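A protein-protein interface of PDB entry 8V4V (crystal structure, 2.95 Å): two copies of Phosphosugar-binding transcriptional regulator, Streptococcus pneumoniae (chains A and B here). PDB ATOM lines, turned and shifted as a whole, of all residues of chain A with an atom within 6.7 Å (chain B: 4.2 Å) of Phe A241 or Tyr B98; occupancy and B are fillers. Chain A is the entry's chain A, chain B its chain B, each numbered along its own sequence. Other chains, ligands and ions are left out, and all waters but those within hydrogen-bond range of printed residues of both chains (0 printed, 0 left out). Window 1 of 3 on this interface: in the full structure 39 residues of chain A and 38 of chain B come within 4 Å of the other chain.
Of the 10 printed residues of chain B, 6 touch a printed residue of chain A.
Printed residues of chain B that touch a printed residue of chain A: Val B94, Leu B95, Tyr B98, Ser B99, Arg B102 and Ile B233.
Hydrophobic or aromatic side chains of chain B that line the printed part of chain A: Val B94, Leu B95, Tyr B98 and Ile B233.
Of the 20 printed residues of chain A, 6 touch a printed residue of chain B.
Along chain A the printed residues that touch a printed residue of chain B span positions 99 to 245.
Ser A99 touches Arg B102, and with the chains exchanged Arg A102 touches Ser B99.
Of the 9 pairs that touch across the chains among the printed residues, 2 have their exchanged pair printed and touching as well.
OH of Tyr B98 is in hydrogen-bond range of OD2 of Asp A244 (2.7 Å).
The side-chain hydroxyl (OH) of Tyr B98 lies close to the backbone NH (N) of Phe A241.
O of Leu A240 lies within hydrogen-bond range of OH of Tyr B98 (2.7 Å).
The guanidinium group of Arg A102 is in hydrogen-bond range of the side-chain hydroxyl of Ser B99 (3.1 Å).
Ser A99 touches Arg B102.
Leu B95 touches Arg A102 (CD2 to CG, 3.8 Å).
CG1 of Val B94 touches CB of Asp A244, 3.9 Å away.
Asp A244 touches Ile B233.
Leu A245 touches Val B94.
Printed residues of chain B within 4 Å of Ser A99: Arg B102.
Phe A241 touches just one residue of chain B: Tyr B98.
Of the printed residues of chain B, Asp A244 touches Val B94, Tyr B98 and Ile B233.
Tyr B98 touches three residues of chain A.
Printed residues of chain A within 4 Å of Ser B99: Arg A102 (3.1 Å).
Of the printed residues of chain A, Ile B233 touches Asp A244.
The nearest printed residue of chain B that does not touch Phe A241 is Leu B95 (4.5 Å).
The nearest printed residue of chain A that does not touch Val B94 is Phe A241 (4.6 Å).
The backbone carbonyl oxygen of Ser A99 is in hydrogen-bond range of the guanidinium group of Arg A102 (3.2 Å).
The guanidinium group of Arg A102 is in salt-bridge range of the side-chain carboxylate of Glu A103 (3.99 Å).
The backbone carbonyl oxygen of Leu B95 sits at hydrogen-bond distance from the side-chain hydroxyl of Ser B99, 3.4 Å away.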
ATOM      1  N   TYR A  98     -14.877  25.547  17.126  1.00  0.00           N
ATOM      2  CA  TYR A  98     -14.377  25.517  18.497  1.00  0.00           C
ATOM      3  C   TYR A  98     -13.894  24.121  18.870  1.00  0.00           C
ATOM      4  O   TYR A  98     -12.799  23.955  19.420  1.00  0.00           O
ATOM      5  CB  TYR A  98     -15.473  25.971  19.461  1.00  0.00           C
ATOM      6  CG  TYR A  98     -15.590  27.469  19.633  1.00  0.00           C
ATOM      7  CD1 TYR A  98     -16.333  28.233  18.744  1.00  0.00           C
ATOM      8  CD2 TYR A  98     -14.976  28.117  20.698  1.00  0.00           C
ATOM      9  CE1 TYR A  98     -16.452  29.603  18.901  1.00  0.00           C
ATOM     10  CE2 TYR A  98     -15.095  29.486  20.866  1.00  0.00           C
ATOM     11  CZ  TYR A  98     -15.828  30.223  19.963  1.00  0.00           C
ATOM     12  OH  TYR A  98     -15.937  31.584  20.134  1.00  0.00           O
ATOM     13  N   SER A  99     -14.703  23.101  18.580  1.00  0.00           N
ATOM     14  CA  SER A  99     -14.299  21.734  18.890  1.00  0.00           C
ATOM     15  C   SER A  99     -12.991  21.381  18.193  1.00  0.00           C
ATOM     16  O   SER A  99     -12.049  20.892  18.828  1.00  0.00           O
ATOM     17  CB  SER A  99     -15.401  20.758  18.482  1.00  0.00           C
ATOM     18  OG  SER A  99     -16.609  21.024  19.173  1.00  0.00           O
ATOM     19  N   MET A 101     -10.740  23.308  17.281  1.00  0.00           N
ATOM     20  CA  MET A 101      -9.645  24.055  17.889  1.00  0.00           C
ATOM     21  C   MET A 101      -9.148  23.371  19.160  1.00  0.00           C
ATOM     22  O   MET A 101      -7.960  23.474  19.489  1.00  0.00           O
ATOM     23  CB  MET A 101     -10.082  25.492  18.184  1.00  0.00           C
ATOM     24  CG  MET A 101      -8.918  26.431  18.463  1.00  0.00           C
ATOM     25  SD  MET A 101      -9.108  28.076  17.752  1.00  0.00           S
ATOM     26  CE  MET A 101      -8.814  27.748  16.015  1.00  0.00           C
ATOM     27  N   ARG A 102     -10.028  22.666  19.882  1.00  0.00           N
ATOM     28  CA  ARG A 102      -9.574  21.925  21.059  1.00  0.00           C
ATOM     29  C   ARG A 102      -8.844  20.654  20.665  1.00  0.00           C
ATOM     30  O   ARG A 102      -7.771  20.356  21.200  1.00  0.00           O
ATOM     31  CB  ARG A 102     -10.743  21.585  21.977  1.00  0.00           C
ATOM     32  CG  ARG A 102     -10.364  20.920  23.333  1.00  0.00           C
ATOM     33  CD  ARG A 102     -10.502  19.386  23.310  1.00  0.00           C
ATOM     34  NE  ARG A 102     -11.782  19.094  22.681  1.00  0.00           N
ATOM     35  CZ  ARG A 102     -11.955  18.242  21.678  1.00  0.00           C
ATOM     36  NH1 ARG A 102     -11.230  17.139  21.584  1.00  0.00           N
ATOM     37  NH2 ARG A 102     -12.901  18.483  20.762  1.00  0.00           N
ATOM     38  N   GLU A 103      -9.404  19.895  19.721  1.00  0.00           N
ATOM     39  CA  GLU A 103      -8.726  18.689  19.264  1.00  0.00           C
ATOM     40  C   GLU A 103      -7.331  19.024  18.756  1.00  0.00           C
ATOM     41  O   GLU A 103      -6.342  18.395  19.152  1.00  0.00           O
ATOM     42  CB  GLU A 103      -9.540  18.005  18.166  1.00  0.00           C
ATOM     43  CG  GLU A 103     -11.018  17.840  18.455  1.00  0.00           C
ATOM     44  CD  GLU A 103     -11.681  16.849  17.517  1.00  0.00           C
ATOM     45  OE1 GLU A 103     -11.113  15.755  17.302  1.00  0.00           O
ATOM     46  OE2 GLU A 103     -12.769  17.170  16.992  1.00  0.00           O
ATOM     47  N   THR A 105      -5.412  21.750  19.300  1.00  0.00           N
ATOM     48  CA  THR A 105      -4.530  22.229  20.357  1.00  0.00           C
ATOM     49  C   THR A 105      -3.982  21.071  21.177  1.00  0.00           C
ATOM     50  O   THR A 105      -2.822  21.092  21.603  1.00  0.00           O
ATOM     51  CB  THR A 105      -5.273  23.215  21.259  1.00  0.00           C
ATOM     52  OG1 THR A 105      -5.398  24.474  20.588  1.00  0.00           O
ATOM     53  CG2 THR A 105      -4.529  23.417  22.571  1.00  0.00           C
ATOM     54  N   GLN A 106      -4.802  20.045  21.404  1.00  0.00           N
ATOM     55  CA  GLN A 106      -4.344  18.906  22.187  1.00  0.00           C
ATOM     56  C   GLN A 106      -3.158  18.217  21.521  1.00  0.00           C
ATOM     57  O   GLN A 106      -2.182  17.864  22.192  1.00  0.00           O
ATOM     58  CB  GLN A 106      -5.494  17.920  22.386  1.00  0.00           C
ATOM     59  CG  GLN A 106      -5.089  16.614  23.040  1.00  0.00           C
ATOM     60  CD  GLN A 106      -5.929  15.439  22.570  1.00  0.00           C
ATOM     61  OE1 GLN A 106      -7.157  15.515  22.523  1.00  0.00           O
ATOM     62  NE2 GLN A 106      -5.264  14.343  22.217  1.00  0.00           N
ATOM     63  N   LEU A 114       5.788  24.058  27.623  1.00  0.00           N
ATOM     64  CA  LEU A 114       4.848  24.929  28.318  1.00  0.00           C
ATOM     65  C   LEU A 114       5.270  25.133  29.766  1.00  0.00           C
ATOM     66  O   LEU A 114       5.306  26.264  30.261  1.00  0.00           O
ATOM     67  CB  LEU A 114       3.442  24.336  28.247  1.00  0.00           C
ATOM     68  CG  LEU A 114       2.877  24.069  26.851  1.00  0.00           C
ATOM     69  CD1 LEU A 114       1.365  23.874  26.919  1.00  0.00           C
ATOM     70  CD2 LEU A 114       3.226  25.192  25.887  1.00  0.00           C
ATOM     71  N   ALA A 222      -2.814  26.455  17.425  1.00  0.00           N
ATOM     72  CA  ALA A 222      -3.664  25.866  16.403  1.00  0.00           C
ATOM     73  C   ALA A 222      -3.965  26.876  15.301  1.00  0.00           C
ATOM     74  O   ALA A 222      -3.903  28.092  15.497  1.00  0.00           O
ATOM     75  CB  ALA A 222      -4.973  25.363  17.012  1.00  0.00           C
ATOM     76  N   GLN A 236      -8.353  35.189  18.866  1.00  0.00           N
ATOM     77  CA  GLN A 236      -7.611  35.044  20.110  1.00  0.00           C
ATOM     78  C   GLN A 236      -7.467  33.585  20.514  1.00  0.00           C
ATOM     79  O   GLN A 236      -6.505  33.222  21.202  1.00  0.00           O
ATOM     80  CB  GLN A 236      -8.308  35.797  21.243  1.00  0.00           C
ATOM     81  CG  GLN A 236      -8.524  37.277  21.031  1.00  0.00           C
ATOM     82  CD  GLN A 236      -9.010  37.963  22.295  1.00  0.00           C
ATOM     83  OE1 GLN A 236      -8.217  38.437  23.107  1.00  0.00           O
ATOM     84  NE2 GLN A 236     -10.324  37.986  22.482  1.00  0.00           N
ATOM     85  N   LEU A 237      -8.408  32.740  20.099  1.00  0.00           N
ATOM     86  CA  LEU A 237      -8.563  31.438  20.743  1.00  0.00           C
ATOM     87  C   LEU A 237      -7.331  30.554  20.635  1.00  0.00           C
ATOM     88  O   LEU A 237      -6.915  29.988  21.662  1.00  0.00           O
ATOM     89  CB  LEU A 237      -9.784  30.725  20.158  1.00  0.00           C
ATOM     90  CG  LEU A 237     -11.125  30.934  20.847  1.00  0.00           C
ATOM     91  CD1 LEU A 237     -11.807  32.142  20.275  1.00  0.00           C
ATOM     92  CD2 LEU A 237     -11.980  29.697  20.665  1.00  0.00           C
ATOM     93  N   PRO A 238      -6.715  30.370  19.465  1.00  0.00           N
ATOM     94  CA  PRO A 238      -5.517  29.516  19.409  1.00  0.00           C
ATOM     95  C   PRO A 238      -4.511  29.847  20.494  1.00  0.00           C
ATOM     96  O   PRO A 238      -3.789  28.958  20.962  1.00  0.00           O
ATOM     97  CB  PRO A 238      -4.955  29.787  18.007  1.00  0.00           C
ATOM     98  CG  PRO A 238      -6.141  30.197  17.201  1.00  0.00           C
ATOM     99  CD  PRO A 238      -7.083  30.908  18.142  1.00  0.00           C
ATOM    100  N   MET A 239      -4.470  31.102  20.930  1.00  0.00           N
ATOM    101  CA  MET A 239      -3.500  31.556  21.915  1.00  0.00           C
ATOM    102  C   MET A 239      -4.037  31.501  23.339  1.00  0.00           C
ATOM    103  O   MET A 239      -3.271  31.241  24.274  1.00  0.00           O
ATOM    104  CB  MET A 239      -3.083  32.985  21.573  1.00  0.00           C
ATOM    105  CG  MET A 239      -2.772  33.168  20.088  1.00  0.00           C
ATOM    106  SD  MET A 239      -1.413  34.304  19.817  1.00  0.00           S
ATOM    107  CE  MET A 239      -0.765  33.717  18.258  1.00  0.00           C
ATOM    108  N   LEU A 240      -5.334  31.743  23.533  1.00  0.00           N
ATOM    109  CA  LEU A 240      -5.892  31.656  24.877  1.00  0.00           C
ATOM    110  C   LEU A 240      -5.835  30.230  25.404  1.00  0.00           C
ATOM    111  O   LEU A 240      -5.802  30.019  26.621  1.00  0.00           O
ATOM    112  CB  LEU A 240      -7.327  32.168  24.883  1.00  0.00           C
ATOM    113  CG  LEU A 240      -7.531  33.649  24.565  1.00  0.00           C
ATOM    114  CD1 LEU A 240      -9.018  33.936  24.414  1.00  0.00           C
ATOM    115  CD2 LEU A 240      -6.918  34.528  25.643  1.00  0.00           C
ATOM    116  N   PHE A 241      -5.830  29.241  24.507  1.00  0.00           N
ATOM    117  CA  PHE A 241      -5.637  27.861  24.940  1.00  0.00           C
ATOM    118  C   PHE A 241      -4.317  27.710  25.682  1.00  0.00           C
ATOM    119  O   PHE A 241      -4.271  27.177  26.798  1.00  0.00           O
ATOM    120  CB  PHE A 241      -5.666  26.916  23.736  1.00  0.00           C
ATOM    121  CG  PHE A 241      -7.027  26.363  23.424  1.00  0.00           C
ATOM    122  CD1 PHE A 241      -7.529  25.274  24.121  1.00  0.00           C
ATOM    123  CD2 PHE A 241      -7.800  26.922  22.418  1.00  0.00           C
ATOM    124  CE1 PHE A 241      -8.787  24.761  23.828  1.00  0.00           C
ATOM    125  CE2 PHE A 241      -9.057  26.416  22.119  1.00  0.00           C
ATOM    126  CZ  PHE A 241      -9.551  25.335  22.822  1.00  0.00           C
ATOM    127  N   PHE A 242      -3.225  28.171  25.068  1.00  0.00           N
ATOM    128  CA  PHE A 242      -1.897  27.958  25.625  1.00  0.00           C
ATOM    129  C   PHE A 242      -1.574  28.941  26.738  1.00  0.00           C
ATOM    130  O   PHE A 242      -0.749  28.634  27.605  1.00  0.00           O
ATOM    131  CB  PHE A 242      -0.857  28.046  24.516  1.00  0.00           C
ATOM    132  CG  PHE A 242      -0.791  26.813  23.673  1.00  0.00           C
ATOM    133  CD1 PHE A 242      -1.734  26.583  22.683  1.00  0.00           C
ATOM    134  CD2 PHE A 242       0.198  25.873  23.877  1.00  0.00           C
ATOM    135  CE1 PHE A 242      -1.684  25.438  21.899  1.00  0.00           C
ATOM    136  CE2 PHE A 242       0.252  24.729  23.098  1.00  0.00           C
ATOM    137  CZ  PHE A 242      -0.694  24.512  22.107  1.00  0.00           C
ATOM    138  N   ILE A 243      -2.208  30.112  26.744  1.00  0.00           N
ATOM    139  CA  ILE A 243      -2.084  31.000  27.896  1.00  0.00           C
ATOM    140  C   ILE A 243      -2.636  30.318  29.142  1.00  0.00           C
ATOM    141  O   ILE A 243      -2.014  30.333  30.211  1.00  0.00           O
ATOM    142  CB  ILE A 243      -2.795  32.337  27.629  1.00  0.00           C
ATOM    143  CG1 ILE A 243      -1.942  33.212  26.713  1.00  0.00           C
ATOM    144  CG2 ILE A 243      -3.080  33.055  28.947  1.00  0.00           C
ATOM    145  CD1 ILE A 243      -2.656  34.434  26.225  1.00  0.00           C
ATOM    146  N   ASP A 244      -3.814  29.704  29.018  1.00  0.00           N
ATOM    147  CA  ASP A 244      -4.442  29.062  30.167  1.00  0.00           C
ATOM    148  C   ASP A 244      -3.647  27.853  30.645  1.00  0.00           C
ATOM    149  O   ASP A 244      -3.652  27.543  31.842  1.00  0.00           O
ATOM    150  CB  ASP A 244      -5.870  28.659  29.812  1.00  0.00           C
ATOM    151  CG  ASP A 244      -6.883  29.695  30.227  1.00  0.00           C
ATOM    152  OD1 ASP A 244      -6.793  30.186  31.376  1.00  0.00           O
ATOM    153  OD2 ASP A 244      -7.777  29.996  29.410  1.00  0.00           O
ATOM    154  N   LEU A 245      -2.966  27.154  29.738  1.00  0.00           N
ATOM    155  CA  LEU A 245      -2.118  26.043  30.154  1.00  0.00           C
ATOM    156  C   LEU A 245      -0.874  26.545  30.873  1.00  0.00           C
ATOM    157  O   LEU A 245      -0.530  26.057  31.955  1.00  0.00           O
ATOM    158  CB  LEU A 245      -1.737  25.198  28.943  1.00  0.00           C
ATOM    159  CG  LEU A 245      -2.882  24.421  28.298  1.00  0.00           C
ATOM    160  CD1 LEU A 245      -2.367  23.750  27.048  1.00  0.00           C
ATOM    161  CD2 LEU A 245      -3.466  23.398  29.254  1.00  0.00           C
ATOM    162  N   ILE A 246      -0.198  27.539  30.295  1.00  0.00           N
ATOM    163  CA  ILE A 246       0.956  28.129  30.966  1.00  0.00           C
ATOM    164  C   ILE A 246       0.532  28.739  32.294  1.00  0.00           C
ATOM    165  O   ILE A 246       1.260  28.665  33.290  1.00  0.00           O
ATOM    166  CB  ILE A 246       1.634  29.174  30.063  1.00  0.00           C
ATOM    167  CG1 ILE A 246       2.310  28.498  28.870  1.00  0.00           C
ATOM    168  CG2 ILE A 246       2.652  29.984  30.862  1.00  0.00           C
ATOM    169  CD1 ILE A 246       2.673  29.462  27.755  1.00  0.00           C
ATOM    170  N   VAL B  94      -7.329  21.859  32.205  1.00  0.00           N
ATOM    171  CA  VAL B  94      -7.671  22.987  31.342  1.00  0.00           C
ATOM    172  C   VAL B  94      -8.521  22.523  30.166  1.00  0.00           C
ATOM    173  O   VAL B  94      -9.565  23.108  29.858  1.00  0.00           O
ATOM    174  CB  VAL B  94      -6.393  23.695  30.859  1.00  0.00           C
ATOM    175  CG1 VAL B  94      -6.740  24.893  29.989  1.00  0.00           C
ATOM    176  CG2 VAL B  94      -5.530  24.112  32.044  1.00  0.00           C
ATOM    177  N   LEU B  95      -8.079  21.463  29.486  1.00  0.00           N
ATOM    178  CA  LEU B  95      -8.775  21.015  28.285  1.00  0.00           C
ATOM    179  C   LEU B  95     -10.205  20.595  28.592  1.00  0.00           C
ATOM    180  O   LEU B  95     -11.091  20.748  27.743  1.00  0.00           O
ATOM    181  CB  LEU B  95      -8.007  19.862  27.641  1.00  0.00           C
ATOM    182  CG  LEU B  95      -6.791  20.268  26.809  1.00  0.00           C
ATOM    183  CD1 LEU B  95      -5.909  19.064  26.516  1.00  0.00           C
ATOM    184  CD2 LEU B  95      -7.229  20.945  25.518  1.00  0.00           C
ATOM    185  N   ARG B  96     -10.449  20.055  29.788  1.00  0.00           N
ATOM    186  CA  ARG B  96     -11.804  19.685  30.172  1.00  0.00           C
ATOM    187  C   ARG B  96     -12.627  20.910  30.542  1.00  0.00           C
ATOM    188  O   ARG B  96     -13.849  20.888  30.399  1.00  0.00           O
ATOM    189  CB  ARG B  96     -11.767  18.696  31.336  1.00  0.00           C
ATOM    190  CG  ARG B  96     -13.049  17.885  31.557  1.00  0.00           C
ATOM    191  CD  ARG B  96     -12.804  16.948  32.734  1.00  0.00           C
ATOM    192  NE  ARG B  96     -12.430  17.791  33.860  1.00  0.00           N
ATOM    193  CZ  ARG B  96     -13.252  18.221  34.805  1.00  0.00           C
ATOM    194  NH1 ARG B  96     -14.374  17.584  35.084  1.00  0.00           N
ATOM    195  NH2 ARG B  96     -12.935  19.320  35.487  1.00  0.00           N
ATOM    196  N   SER B  97     -11.990  21.984  31.015  1.00  0.00           N
ATOM    197  CA  SER B  97     -12.717  23.236  31.197  1.00  0.00           C
ATOM    198  C   SER B  97     -13.174  23.798  29.857  1.00  0.00           C
ATOM    199  O   SER B  97     -14.268  24.364  29.752  1.00  0.00           O
ATOM    200  CB  SER B  97     -11.842  24.251  31.934  1.00  0.00           C
ATOM    201  OG  SER B  97     -11.704  23.922  33.308  1.00  0.00           O
ATOM    202  N   TYR B  98     -12.334  23.669  28.828  1.00  0.00           N
ATOM    203  CA  TYR B  98     -12.685  24.166  27.502  1.00  0.00           C
ATOM    204  C   TYR B  98     -13.809  23.342  26.885  1.00  0.00           C
ATOM    205  O   TYR B  98     -14.813  23.893  26.421  1.00  0.00           O
ATOM    206  CB  TYR B  98     -11.453  24.145  26.600  1.00  0.00           C
ATOM    207  CG  TYR B  98     -10.578  25.368  26.722  1.00  0.00           C
ATOM    208  CD1 TYR B  98      -9.587  25.442  27.692  1.00  0.00           C
ATOM    209  CD2 TYR B  98     -10.735  26.446  25.860  1.00  0.00           C
ATOM    210  CE1 TYR B  98      -8.780  26.559  27.804  1.00  0.00           C
ATOM    211  CE2 TYR B  98      -9.934  27.564  25.963  1.00  0.00           C
ATOM    212  CZ  TYR B  98      -8.959  27.617  26.937  1.00  0.00           C
ATOM    213  OH  TYR B  98      -8.164  28.734  27.038  1.00  0.00           O
ATOM    214  N   SER B  99     -13.661  22.016  26.880  1.00  0.00           N
ATOM    215  CA  SER B  99     -14.715  21.168  26.332  1.00  0.00           C
ATOM    216  C   SER B  99     -16.014  21.356  27.105  1.00  0.00           C
ATOM    217  O   SER B  99     -17.090  21.511  26.513  1.00  0.00           O
ATOM    218  CB  SER B  99     -14.279  19.704  26.364  1.00  0.00           C
ATOM    219  OG  SER B  99     -13.212  19.461  25.463  1.00  0.00           O
ATOM    220  N   ASN B 100     -15.927  21.351  28.438  1.00  0.00           N
ATOM    221  CA  ASN B 100     -17.105  21.584  29.267  1.00  0.00           C
ATOM    222  C   ASN B 100     -17.810  22.869  28.858  1.00  0.00           C
ATOM    223  O   ASN B 100     -19.042  22.912  28.760  1.00  0.00           O
ATOM    224  CB  ASN B 100     -16.701  21.647  30.740  1.00  0.00           C
ATOM    225  CG  ASN B 100     -17.702  20.969  31.648  1.00  0.00           C
ATOM    226  OD1 ASN B 100     -18.357  20.004  31.258  1.00  0.00           O
ATOM    227  ND2 ASN B 100     -17.853  21.492  32.861  1.00  0.00           N
ATOM    228  N   MET B 101     -17.041  23.929  28.599  1.00  0.00           N
ATOM    229  CA  MET B 101     -17.638  25.196  28.196  1.00  0.00           C
ATOM    230  C   MET B 101     -18.417  25.045  26.900  1.00  0.00           C
ATOM    231  O   MET B 101     -19.599  25.401  26.825  1.00  0.00           O
ATOM    232  CB  MET B 101     -16.551  26.254  28.033  1.00  0.00           C
ATOM    233  CG  MET B 101     -17.085  27.655  27.809  1.00  0.00           C
ATOM    234  SD  MET B 101     -16.988  28.638  29.309  1.00  0.00           S
ATOM    235  CE  MET B 101     -15.238  29.023  29.324  1.00  0.00           C
ATOM    236  N   ARG B 102     -17.770  24.503  25.865  1.00  0.00           N
ATOM    237  CA  ARG B 102     -18.465  24.328  24.597  1.00  0.00           C
ATOM    238  C   ARG B 102     -19.735  23.515  24.789  1.00  0.00           C
ATOM    239  O   ARG B 102     -20.786  23.858  24.235  1.00  0.00           O
ATOM    240  CB  ARG B 102     -17.553  23.653  23.573  1.00  0.00           C
ATOM    241  CG  ARG B 102     -18.291  23.185  22.325  1.00  0.00           C
ATOM    242  CD  ARG B 102     -17.730  21.883  21.767  1.00  0.00           C
ATOM    243  NE  ARG B 102     -17.672  20.814  22.759  1.00  0.00           N
ATOM    244  CZ  ARG B 102     -18.697  20.038  23.085  1.00  0.00           C
ATOM    245  NH1 ARG B 102     -19.896  20.211  22.553  1.00  0.00           N
ATOM    246  NH2 ARG B 102     -18.515  19.064  23.972  1.00  0.00           N
ATOM    247  N   ILE B 233     -10.268  29.215  33.963  1.00  0.00           N
ATOM    248  CA  ILE B 233      -9.635  29.590  32.706  1.00  0.00           C
ATOM    249  C   ILE B 233     -10.185  30.950  32.300  1.00  0.00           C
ATOM    250  O   ILE B 233     -11.109  31.466  32.941  1.00  0.00           O
ATOM    251  CB  ILE B 233      -9.861  28.526  31.616  1.00  0.00           C
ATOM    252  CG1 ILE B 233     -11.267  28.610  31.033  1.00  0.00           C
ATOM    253  CG2 ILE B 233      -9.593  27.129  32.153  1.00  0.00           C
ATOM    254  CD1 ILE B 233     -11.386  27.930  29.658  1.00  0.00           C
